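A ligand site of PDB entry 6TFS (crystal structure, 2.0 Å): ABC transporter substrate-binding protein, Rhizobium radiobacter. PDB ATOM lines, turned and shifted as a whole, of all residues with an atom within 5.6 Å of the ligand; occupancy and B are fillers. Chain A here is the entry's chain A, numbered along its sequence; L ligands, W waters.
The backbone carbonyl oxygen (O) of Gly 341 lies within hydrogen-bond range of the guanidinium group (NH2) of Arg 284 (2.9 Å). The side-chain amide nitrogen (ND2) of Asn 251 lies within hydrogen-bond range of the side-chain amide oxygen (OD1) of Asn 460, 2.8 Å away. OG of Ser 344 is in hydrogen-bond range of O of Gly 341, at 3.0 Å. A ring nitrogen (ND1) of His 371 sits at hydrogen-bond distance from the guanidinium group (NH1) of Arg 375 (2.9 Å). The guanidinium group (NH2) of Arg 375 sits at hydrogen-bond distance from the side-chain hydroxyl (OH) of Tyr 384, at 2.9 Å. A ring nitrogen (NE2) of His 367 is in hydrogen-bond range of a ring nitrogen (NE2) of His 371, at 3.2 Å. The backbone NH (N) of Glu 249 is in hydrogen-bond range of the backbone carbonyl oxygen (O) of Asn 460, 2.8 Å away. The backbone carbonyl oxygen (O) of Ala 386 is in hydrogen-bond range of the backbone NH (N) of Leu 250 (2.9 Å).
Water W3 lies within hydrogen-bond range of an oxygen (O8) of the ligand (2.7 Å) and the guanidinium group (NE) of Arg 29 (3.0 Å). Water W2 bridges an oxygen (O9) of the ligand (2.8 Å) and the backbone NH (N) of Gly 385 (3.0 Å). Water W1 lies within hydrogen-bond range of OE1 of Glu 249, OG1 of Thr 26 and O4 of the ligand.
An oxygen (O8) of the ligand lies close to the backbone carbonyl oxygen (O) of Thr 24 (3.3 Å). O5 of the ligand sits close to O of Gly 385, at 3.2 Å. Residues that only touch the ligand: Thr 25 (3.5 Å), Leu 339 (3.8 Å) and Ala 386 (3.8 Å). Hydrophobic or aromatic side chains within 4 Å of the ligand: Leu 339, Leu 342, His 367, His 371 and Tyr 384. Of the 28 residues printed, 18 come within 4 Å of the ligand. Along chain A the residues within 4 Å of the ligand span positions 24 to 460. The nearest printed residue that does not touch the ligand is Leu 345 (4.2 Å).
The side-chain amide nitrogen (ND2) of Asn 460 lies within hydrogen-bond range of an oxygen (O3) of the ligand (3.2 Å). An oxygen (O7) of the ligand lies within hydrogen-bond range of the side-chain hydroxyl (OH) of Tyr 384. N of Leu 342 is in hydrogen-bond range of O2 of the ligand. NH2 of Arg 388 lies within salt-bridge range of O7 of the ligand (2.8 Å). OD1 of Asn 251 sits at hydrogen-bond distance from O3 of the ligand (2.7 Å). The side-chain hydroxyl (OG1) of Thr 26 lies within hydrogen-bond range of a nitrogen (N1) of the ligand, at 2.8 Å. OE1 of Gln 226 is in hydrogen-bond range of O1 of the ligand, 2.9 Å away. O6 of the ligand lies within hydrogen-bond range of NE2 of His 367 (2.8 Å). OE2 of Glu 249 is in salt-bridge range of N1 of the ligand (2.8 Å). O8 of the ligand lies within salt-bridge range of NH2 of Arg 29 (3.1 Å). An oxygen (O9) of the ligand sits at hydrogen-bond distance from a ring nitrogen (NE2) of His 371, 2.8 Å away. N of Thr 26 sits at hydrogen-bond distance from O6 of the ligand (3.1 Å). The guanidinium group (NH1) of Arg 284 is in hydrogen-bond range of an oxygen (O1) of the ligand (2.8 Å). The backbone carbonyl oxygen (O) of Gly 341 is in hydrogen-bond range of an oxygen (O1) of the ligand.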
ATOM      1  N   THR A  24       0.902 -14.598 -11.504  1.00  0.00           N
ATOM      2  CA  THR A  24       1.322 -15.969 -11.204  1.00  0.00           C
ATOM      3  C   THR A  24       2.301 -16.548 -12.224  1.00  0.00           C
ATOM      4  O   THR A  24       3.237 -17.243 -11.818  1.00  0.00           O
ATOM      5  CB  THR A  24       0.075 -16.865 -11.030  1.00  0.00           C
ATOM      6  OG1 THR A  24      -0.744 -16.314  -9.993  1.00  0.00           O
ATOM      7  CG2 THR A  24       0.434 -18.327 -10.690  1.00  0.00           C
ATOM      8  N   THR A  25       2.068 -16.327 -13.514  1.00  0.00           N
ATOM      9  CA  THR A  25       2.977 -16.828 -14.545  1.00  0.00           C
ATOM     10  C   THR A  25       4.333 -16.127 -14.373  1.00  0.00           C
ATOM     11  O   THR A  25       4.370 -14.968 -13.912  1.00  0.00           O
ATOM     12  CB  THR A  25       2.421 -16.617 -15.971  1.00  0.00           C
ATOM     13  OG1 THR A  25       2.392 -15.214 -16.271  1.00  0.00           O
ATOM     14  CG2 THR A  25       1.045 -17.265 -16.195  1.00  0.00           C
ATOM     15  N   THR A  26       5.425 -16.803 -14.756  1.00  0.00           N
ATOM     16  CA  THR A  26       6.766 -16.231 -14.684  1.00  0.00           C
ATOM     17  C   THR A  26       6.799 -14.845 -15.347  1.00  0.00           C
ATOM     18  O   THR A  26       7.332 -13.911 -14.765  1.00  0.00           O
ATOM     19  CB  THR A  26       7.817 -17.166 -15.288  1.00  0.00           C
ATOM     20  OG1 THR A  26       7.968 -18.273 -14.399  1.00  0.00           O
ATOM     21  CG2 THR A  26       9.188 -16.480 -15.500  1.00  0.00           C
ATOM     22  N   SER A  27       6.211 -14.724 -16.550  1.00  0.00           N
ATOM     23  CA  SER A  27       6.194 -13.465 -17.289  1.00  0.00           C
ATOM     24  C   SER A  27       5.480 -12.319 -16.546  1.00  0.00           C
ATOM     25  O   SER A  27       6.049 -11.237 -16.455  1.00  0.00           O
ATOM     26  CB  SER A  27       5.631 -13.667 -18.692  1.00  0.00           C
ATOM     27  OG  SER A  27       5.843 -12.517 -19.477  1.00  0.00           O
ATOM     28  N   ARG A  29       4.932 -12.152 -13.232  1.00  0.00           N
ATOM     29  CA  ARG A  29       5.753 -11.941 -12.024  1.00  0.00           C
ATOM     30  C   ARG A  29       7.010 -11.132 -12.317  1.00  0.00           C
ATOM     31  O   ARG A  29       7.402 -10.308 -11.506  1.00  0.00           O
ATOM     32  CB  ARG A  29       6.149 -13.278 -11.370  1.00  0.00           C
ATOM     33  CG  ARG A  29       4.979 -14.057 -10.766  1.00  0.00           C
ATOM     34  CD  ARG A  29       5.569 -15.280 -10.117  1.00  0.00           C
ATOM     35  NE  ARG A  29       4.584 -16.220  -9.605  1.00  0.00           N
ATOM     36  CZ  ARG A  29       4.067 -16.190  -8.385  1.00  0.00           C
ATOM     37  NH1 ARG A  29       4.406 -15.226  -7.536  1.00  0.00           N
ATOM     38  NH2 ARG A  29       3.211 -17.133  -8.002  1.00  0.00           N
ATOM     39  N   GLN A 226      15.668 -25.389 -20.755  1.00  0.00           N
ATOM     40  CA  GLN A 226      16.352 -26.273 -19.782  1.00  0.00           C
ATOM     41  C   GLN A 226      17.370 -27.231 -20.399  1.00  0.00           C
ATOM     42  O   GLN A 226      17.913 -28.077 -19.701  1.00  0.00           O
ATOM     43  CB  GLN A 226      15.311 -27.048 -18.936  1.00  0.00           C
ATOM     44  CG  GLN A 226      14.422 -26.161 -18.055  1.00  0.00           C
ATOM     45  CD  GLN A 226      13.362 -25.401 -18.846  1.00  0.00           C
ATOM     46  OE1 GLN A 226      12.654 -25.962 -19.682  1.00  0.00           O
ATOM     47  NE2 GLN A 226      13.256 -24.111 -18.597  1.00  0.00           N
ATOM     48  N   GLU A 249      13.088 -23.985 -10.147  1.00  0.00           N
ATOM     49  CA  GLU A 249      11.649 -24.250 -10.086  1.00  0.00           C
ATOM     50  C   GLU A 249      11.408 -25.739 -10.171  1.00  0.00           C
ATOM     51  O   GLU A 249      11.907 -26.393 -11.084  1.00  0.00           O
ATOM     52  CB  GLU A 249      10.881 -23.494 -11.184  1.00  0.00           C
ATOM     53  CG  GLU A 249      10.926 -21.993 -11.008  1.00  0.00           C
ATOM     54  CD  GLU A 249      10.288 -21.263 -12.173  1.00  0.00           C
ATOM     55  OE1 GLU A 249      10.918 -21.202 -13.246  1.00  0.00           O
ATOM     56  OE2 GLU A 249       9.135 -20.791 -12.023  1.00  0.00           O
ATOM     57  N   LEU A 250      10.683 -26.293  -9.189  1.00  0.00           N
ATOM     58  CA  LEU A 250      10.404 -27.721  -9.151  1.00  0.00           C
ATOM     59  C   LEU A 250       9.162 -28.112  -9.976  1.00  0.00           C
ATOM     60  O   LEU A 250       8.094 -27.548  -9.801  1.00  0.00           O
ATOM     61  CB  LEU A 250      10.288 -28.226  -7.701  1.00  0.00           C
ATOM     62  CG  LEU A 250       9.874 -29.699  -7.491  1.00  0.00           C
ATOM     63  CD1 LEU A 250      10.892 -30.693  -8.108  1.00  0.00           C
ATOM     64  CD2 LEU A 250       9.616 -29.994  -6.040  1.00  0.00           C
ATOM     65  N   ASN A 251       9.329 -29.127 -10.829  1.00  0.00           N
ATOM     66  CA  ASN A 251       8.269 -29.701 -11.638  1.00  0.00           C
ATOM     67  C   ASN A 251       7.796 -30.991 -11.009  1.00  0.00           C
ATOM     68  O   ASN A 251       8.615 -31.835 -10.642  1.00  0.00           O
ATOM     69  CB  ASN A 251       8.742 -29.972 -13.056  1.00  0.00           C
ATOM     70  CG  ASN A 251       9.345 -28.783 -13.728  1.00  0.00           C
ATOM     71  OD1 ASN A 251       8.636 -27.871 -14.137  1.00  0.00           O
ATOM     72  ND2 ASN A 251      10.641 -28.793 -13.936  1.00  0.00           N
ATOM     73  N   ARG A 284      18.541 -33.423 -19.944  1.00  0.00           N
ATOM     74  CA  ARG A 284      18.509 -31.963 -20.021  1.00  0.00           C
ATOM     75  C   ARG A 284      19.861 -31.281 -19.703  1.00  0.00           C
ATOM     76  O   ARG A 284      20.226 -30.310 -20.356  1.00  0.00           O
ATOM     77  CB  ARG A 284      17.379 -31.413 -19.149  1.00  0.00           C
ATOM     78  CG  ARG A 284      16.002 -31.623 -19.771  1.00  0.00           C
ATOM     79  CD  ARG A 284      14.906 -31.047 -18.911  1.00  0.00           C
ATOM     80  NE  ARG A 284      13.772 -30.680 -19.752  1.00  0.00           N
ATOM     81  CZ  ARG A 284      12.742 -29.948 -19.372  1.00  0.00           C
ATOM     82  NH1 ARG A 284      12.652 -29.512 -18.129  1.00  0.00           N
ATOM     83  NH2 ARG A 284      11.790 -29.650 -20.242  1.00  0.00           N
ATOM     84  N   LEU A 339       3.836 -23.629 -22.689  1.00  0.00           N
ATOM     85  CA  LEU A 339       5.089 -22.988 -22.272  1.00  0.00           C
ATOM     86  C   LEU A 339       6.139 -24.040 -22.768  1.00  0.00           C
ATOM     87  O   LEU A 339       5.938 -25.234 -22.471  1.00  0.00           O
ATOM     88  CB  LEU A 339       5.163 -22.843 -20.730  1.00  0.00           C
ATOM     89  CG  LEU A 339       6.477 -22.260 -20.171  1.00  0.00           C
ATOM     90  CD1 LEU A 339       6.675 -20.822 -20.613  1.00  0.00           C
ATOM     91  CD2 LEU A 339       6.547 -22.400 -18.651  1.00  0.00           C
ATOM     92  N   PRO A 340       7.094 -23.691 -23.673  1.00  0.00           N
ATOM     93  CA  PRO A 340       7.943 -24.722 -24.303  1.00  0.00           C
ATOM     94  C   PRO A 340       8.652 -25.705 -23.376  1.00  0.00           C
ATOM     95  O   PRO A 340       8.697 -26.902 -23.704  1.00  0.00           O
ATOM     96  CB  PRO A 340       8.944 -23.906 -25.140  1.00  0.00           C
ATOM     97  CG  PRO A 340       8.172 -22.654 -25.476  1.00  0.00           C
ATOM     98  CD  PRO A 340       7.384 -22.345 -24.237  1.00  0.00           C
ATOM     99  N   GLY A 341       9.152 -25.239 -22.236  1.00  0.00           N
ATOM    100  CA  GLY A 341       9.812 -26.085 -21.255  1.00  0.00           C
ATOM    101  C   GLY A 341       8.880 -27.137 -20.671  1.00  0.00           C
ATOM    102  O   GLY A 341       9.258 -28.292 -20.532  1.00  0.00           O
ATOM    103  N   LEU A 342       7.634 -26.732 -20.343  1.00  0.00           N
ATOM    104  CA  LEU A 342       6.607 -27.645 -19.824  1.00  0.00           C
ATOM    105  C   LEU A 342       6.139 -28.614 -20.915  1.00  0.00           C
ATOM    106  O   LEU A 342       5.872 -29.783 -20.616  1.00  0.00           O
ATOM    107  CB  LEU A 342       5.409 -26.899 -19.194  1.00  0.00           C
ATOM    108  CG  LEU A 342       5.626 -26.295 -17.787  1.00  0.00           C
ATOM    109  CD1 LEU A 342       4.470 -25.364 -17.395  1.00  0.00           C
ATOM    110  CD2 LEU A 342       5.826 -27.392 -16.713  1.00  0.00           C
ATOM    111  N   SER A 344       8.006 -29.753 -23.614  1.00  0.00           N
ATOM    112  CA  SER A 344       9.076 -30.715 -23.834  1.00  0.00           C
ATOM    113  C   SER A 344       9.147 -31.703 -22.667  1.00  0.00           C
ATOM    114  O   SER A 344       9.358 -32.882 -22.898  1.00  0.00           O
ATOM    115  CB  SER A 344      10.418 -30.029 -24.068  1.00  0.00           C
ATOM    116  OG  SER A 344      10.779 -29.185 -22.995  1.00  0.00           O
ATOM    117  N   LEU A 345       8.930 -31.217 -21.428  1.00  0.00           N
ATOM    118  CA  LEU A 345       8.925 -32.058 -20.239  1.00  0.00           C
ATOM    119  C   LEU A 345       7.791 -33.094 -20.283  1.00  0.00           C
ATOM    120  O   LEU A 345       8.055 -34.270 -20.067  1.00  0.00           O
ATOM    121  CB  LEU A 345       8.899 -31.220 -18.941  1.00  0.00           C
ATOM    122  CG  LEU A 345       8.964 -31.983 -17.612  1.00  0.00           C
ATOM    123  CD1 LEU A 345      10.231 -32.918 -17.528  1.00  0.00           C
ATOM    124  CD2 LEU A 345       8.918 -31.015 -16.450  1.00  0.00           C
ATOM    125  N   HIS A 367      -0.342 -21.438 -22.204  1.00  0.00           N
ATOM    126  CA  HIS A 367       0.071 -21.372 -20.789  1.00  0.00           C
ATOM    127  C   HIS A 367      -0.906 -20.671 -19.827  1.00  0.00           C
ATOM    128  O   HIS A 367      -1.333 -21.293 -18.853  1.00  0.00           O
ATOM    129  CB  HIS A 367       1.482 -20.764 -20.690  1.00  0.00           C
ATOM    130  CG  HIS A 367       2.106 -20.882 -19.337  1.00  0.00           C
ATOM    131  ND1 HIS A 367       2.284 -22.113 -18.727  1.00  0.00           N
ATOM    132  CD2 HIS A 367       2.604 -19.907 -18.532  1.00  0.00           C
ATOM    133  CE1 HIS A 367       2.909 -21.855 -17.587  1.00  0.00           C
ATOM    134  NE2 HIS A 367       3.117 -20.537 -17.431  1.00  0.00           N
ATOM    135  N   TRP A 370      -4.250 -22.407 -19.798  1.00  0.00           N
ATOM    136  CA  TRP A 370      -3.986 -23.660 -19.078  1.00  0.00           C
ATOM    137  C   TRP A 370      -3.986 -23.428 -17.552  1.00  0.00           C
ATOM    138  O   TRP A 370      -4.564 -24.233 -16.815  1.00  0.00           O
ATOM    139  CB  TRP A 370      -2.663 -24.272 -19.564  1.00  0.00           C
ATOM    140  CG  TRP A 370      -2.157 -25.399 -18.727  1.00  0.00           C
ATOM    141  CD1 TRP A 370      -2.501 -26.724 -18.833  1.00  0.00           C
ATOM    142  CD2 TRP A 370      -1.164 -25.323 -17.682  1.00  0.00           C
ATOM    143  NE1 TRP A 370      -1.779 -27.473 -17.941  1.00  0.00           N
ATOM    144  CE2 TRP A 370      -0.952 -26.640 -17.222  1.00  0.00           C
ATOM    145  CE3 TRP A 370      -0.397 -24.276 -17.138  1.00  0.00           C
ATOM    146  CZ2 TRP A 370      -0.023 -26.934 -16.207  1.00  0.00           C
ATOM    147  CZ3 TRP A 370       0.543 -24.574 -16.152  1.00  0.00           C
ATOM    148  CH2 TRP A 370       0.725 -25.900 -15.703  1.00  0.00           C
ATOM    149  N   HIS A 371      -3.385 -22.286 -17.090  1.00  0.00           N
ATOM    150  CA  HIS A 371      -3.364 -21.928 -15.670  1.00  0.00           C
ATOM    151  C   HIS A 371      -4.800 -21.839 -15.079  1.00  0.00           C
ATOM    152  O   HIS A 371      -5.017 -22.278 -13.948  1.00  0.00           O
ATOM    153  CB  HIS A 371      -2.588 -20.603 -15.422  1.00  0.00           C
ATOM    154  CG  HIS A 371      -1.144 -20.821 -15.082  1.00  0.00           C
ATOM    155  ND1 HIS A 371      -0.757 -21.066 -13.792  1.00  0.00           N
ATOM    156  CD2 HIS A 371      -0.057 -20.831 -15.888  1.00  0.00           C
ATOM    157  CE1 HIS A 371       0.562 -21.195 -13.838  1.00  0.00           C
ATOM    158  NE2 HIS A 371       1.021 -21.070 -15.072  1.00  0.00           N
ATOM    159  N   ARG A 375      -7.082 -24.873 -12.552  1.00  0.00           N
ATOM    160  CA  ARG A 375      -7.702 -24.280 -11.369  1.00  0.00           C
ATOM    161  C   ARG A 375      -9.240 -24.464 -11.366  1.00  0.00           C
ATOM    162  O   ARG A 375      -9.904 -24.001 -10.441  1.00  0.00           O
ATOM    163  CB  ARG A 375      -7.266 -22.811 -11.205  1.00  0.00           C
ATOM    164  CG  ARG A 375      -5.870 -22.671 -10.571  1.00  0.00           C
ATOM    165  CD  ARG A 375      -5.353 -21.248 -10.744  1.00  0.00           C
ATOM    166  NE  ARG A 375      -4.016 -21.035 -10.151  1.00  0.00           N
ATOM    167  CZ  ARG A 375      -2.855 -21.310 -10.748  1.00  0.00           C
ATOM    168  NH1 ARG A 375      -2.825 -21.903 -11.938  1.00  0.00           N
ATOM    169  NH2 ARG A 375      -1.712 -21.031 -10.146  1.00  0.00           N
ATOM    170  N   TYR A 384       3.049 -29.229 -13.172  1.00  0.00           N
ATOM    171  CA  TYR A 384       3.242 -27.859 -12.692  1.00  0.00           C
ATOM    172  C   TYR A 384       4.684 -27.606 -12.244  1.00  0.00           C
ATOM    173  O   TYR A 384       5.278 -28.435 -11.571  1.00  0.00           O
ATOM    174  CB  TYR A 384       2.277 -27.594 -11.508  1.00  0.00           C
ATOM    175  CG  TYR A 384       1.936 -26.129 -11.315  1.00  0.00           C
ATOM    176  CD1 TYR A 384       0.865 -25.549 -11.995  1.00  0.00           C
ATOM    177  CD2 TYR A 384       2.664 -25.330 -10.447  1.00  0.00           C
ATOM    178  CE1 TYR A 384       0.534 -24.205 -11.822  1.00  0.00           C
ATOM    179  CE2 TYR A 384       2.345 -23.984 -10.254  1.00  0.00           C
ATOM    180  CZ  TYR A 384       1.276 -23.431 -10.945  1.00  0.00           C
ATOM    181  OH  TYR A 384       0.941 -22.107 -10.788  1.00  0.00           O
ATOM    182  N   GLY A 385       5.203 -26.432 -12.607  1.00  0.00           N
ATOM    183  CA  GLY A 385       6.541 -25.996 -12.219  1.00  0.00           C
ATOM    184  C   GLY A 385       6.481 -24.745 -11.369  1.00  0.00           C
ATOM    185  O   GLY A 385       5.763 -23.817 -11.722  1.00  0.00           O
ATOM    186  N   ALA A 386       7.205 -24.742 -10.224  1.00  0.00           N
ATOM    187  CA  ALA A 386       7.224 -23.583  -9.319  1.00  0.00           C
ATOM    188  C   ALA A 386       8.303 -23.632  -8.252  1.00  0.00           C
ATOM    189  O   ALA A 386       8.699 -24.710  -7.802  1.00  0.00           O
ATOM    190  CB  ALA A 386       5.856 -23.396  -8.628  1.00  0.00           C
ATOM    191  N   ALA A 387       8.702 -22.441  -7.812  1.00  0.00           N
ATOM    192  CA  ALA A 387       9.540 -22.199  -6.641  1.00  0.00           C
ATOM    193  C   ALA A 387       8.707 -21.248  -5.766  1.00  0.00           C
ATOM    194  O   ALA A 387       7.902 -20.465  -6.284  1.00  0.00           O
ATOM    195  CB  ALA A 387      10.864 -21.554  -7.024  1.00  0.00           C
ATOM    196  N   ARG A 388       8.864 -21.359  -4.455  1.00  0.00           N
ATOM    197  CA  ARG A 388       8.191 -20.472  -3.503  1.00  0.00           C
ATOM    198  C   ARG A 388       9.258 -19.931  -2.567  1.00  0.00           C
ATOM    199  O   ARG A 388      10.408 -20.349  -2.692  1.00  0.00           O
ATOM    200  CB  ARG A 388       7.063 -21.207  -2.744  1.00  0.00           C
ATOM    201  CG  ARG A 388       5.801 -21.468  -3.605  1.00  0.00           C
ATOM    202  CD  ARG A 388       5.197 -20.192  -4.153  1.00  0.00           C
ATOM    203  NE  ARG A 388       3.962 -20.390  -4.919  1.00  0.00           N
ATOM    204  CZ  ARG A 388       3.871 -20.382  -6.246  1.00  0.00           C
ATOM    205  NH1 ARG A 388       4.957 -20.205  -6.998  1.00  0.00           N
ATOM    206  NH2 ARG A 388       2.696 -20.528  -6.831  1.00  0.00           N
ATOM    207  N   PHE A 399       0.537 -26.322  -2.123  1.00  0.00           N
ATOM    208  CA  PHE A 399       0.366 -27.480  -2.965  1.00  0.00           C
ATOM    209  C   PHE A 399      -0.276 -28.696  -2.309  1.00  0.00           C
ATOM    210  O   PHE A 399      -0.820 -29.513  -3.044  1.00  0.00           O
ATOM    211  CB  PHE A 399       1.723 -27.884  -3.583  1.00  0.00           C
ATOM    212  CG  PHE A 399       2.224 -26.943  -4.645  1.00  0.00           C
ATOM    213  CD1 PHE A 399       1.840 -27.083  -5.978  1.00  0.00           C
ATOM    214  CD2 PHE A 399       3.096 -25.898  -4.322  1.00  0.00           C
ATOM    215  CE1 PHE A 399       2.326 -26.230  -6.966  1.00  0.00           C
ATOM    216  CE2 PHE A 399       3.582 -25.045  -5.309  1.00  0.00           C
ATOM    217  CZ  PHE A 399       3.195 -25.207  -6.633  1.00  0.00           C
ATOM    218  N   VAL A 413      -2.912 -24.122  -5.126  1.00  0.00           N
ATOM    219  CA  VAL A 413      -2.372 -24.965  -6.187  1.00  0.00           C
ATOM    220  C   VAL A 413      -2.343 -26.440  -5.790  1.00  0.00           C
ATOM    221  O   VAL A 413      -1.510 -27.199  -6.277  1.00  0.00           O
ATOM    222  CB  VAL A 413      -0.984 -24.432  -6.674  1.00  0.00           C
ATOM    223  CG1 VAL A 413      -1.163 -23.236  -7.606  1.00  0.00           C
ATOM    224  CG2 VAL A 413      -0.084 -24.057  -5.492  1.00  0.00           C
ATOM    225  N   ASN A 460      14.579 -26.838 -12.082  1.00  0.00           N
ATOM    226  CA  ASN A 460      15.439 -26.137 -13.024  1.00  0.00           C
ATOM    227  C   ASN A 460      15.702 -24.728 -12.641  1.00  0.00           C
ATOM    228  O   ASN A 460      14.761 -23.986 -12.331  1.00  0.00           O
ATOM    229  CB  ASN A 460      14.883 -26.183 -14.468  1.00  0.00           C
ATOM    230  CG  ASN A 460      13.368 -26.156 -14.604  1.00  0.00           C
ATOM    231  OD1 ASN A 460      12.748 -27.194 -14.855  1.00  0.00           O
ATOM    232  ND2 ASN A 460      12.750 -25.000 -14.422  1.00  0.00           N
HETATM  233  O1  LIG L   1      10.827 -27.450 -18.000  1.00  0.00           O
HETATM  234  C1  LIG L   1       9.773 -26.981 -17.199  1.00  0.00           C
HETATM  235  C2  LIG L   1       9.940 -25.482 -17.044  1.00  0.00           C
HETATM  236  O2  LIG L   1       9.645 -24.836 -18.258  1.00  0.00           O
HETATM  237  C3  LIG L   1       9.083 -24.942 -15.887  1.00  0.00           C
HETATM  238  O3  LIG L   1       9.581 -25.408 -14.645  1.00  0.00           O
HETATM  239  C4  LIG L   1       9.038 -23.420 -15.874  1.00  0.00           C
HETATM  240  O4  LIG L   1      10.287 -22.838 -15.707  1.00  0.00           O
HETATM  241  C5  LIG L   1       8.225 -22.826 -14.733  1.00  0.00           C
HETATM  242  O5  LIG L   1       8.264 -23.272 -13.577  1.00  0.00           O
HETATM  243  C6  LIG L   1       7.422 -21.547 -15.078  1.00  0.00           C
HETATM  244  N1  LIG L   1       7.045 -20.819 -13.890  1.00  0.00           N
HETATM  245  C7  LIG L   1       5.678 -21.107 -13.480  1.00  0.00           C
HETATM  246  C8  LIG L   1       4.655 -20.819 -14.564  1.00  0.00           C
HETATM  247  O6  LIG L   1       4.692 -19.774 -15.218  1.00  0.00           O
HETATM  248  C9  LIG L   1       5.384 -20.339 -12.206  1.00  0.00           C
HETATM  249  C10 LIG L   1       4.034 -20.779 -11.552  1.00  0.00           C
HETATM  250  C11 LIG L   1       3.762 -20.198 -10.204  1.00  0.00           C
HETATM  251  O7  LIG L   1       2.727 -20.566  -9.591  1.00  0.00           O
HETATM  252  O8  LIG L   1       4.536 -19.371  -9.648  1.00  0.00           O
HETATM  253  O9  LIG L   1       3.760 -21.672 -14.788  1.00  0.00           O
HETATM  254  O   HOH W   1      10.530 -19.490 -15.222  1.00  0.00           O
HETATM  255  O   HOH W   2       3.535 -24.313 -13.971  1.00  0.00           O
HETATM  256  O   HOH W   3       6.938 -18.077  -9.629  1.00  0.00           O
HETATM  257  O   HOH W   4      10.404 -21.960 -18.929  1.00  0.00           O
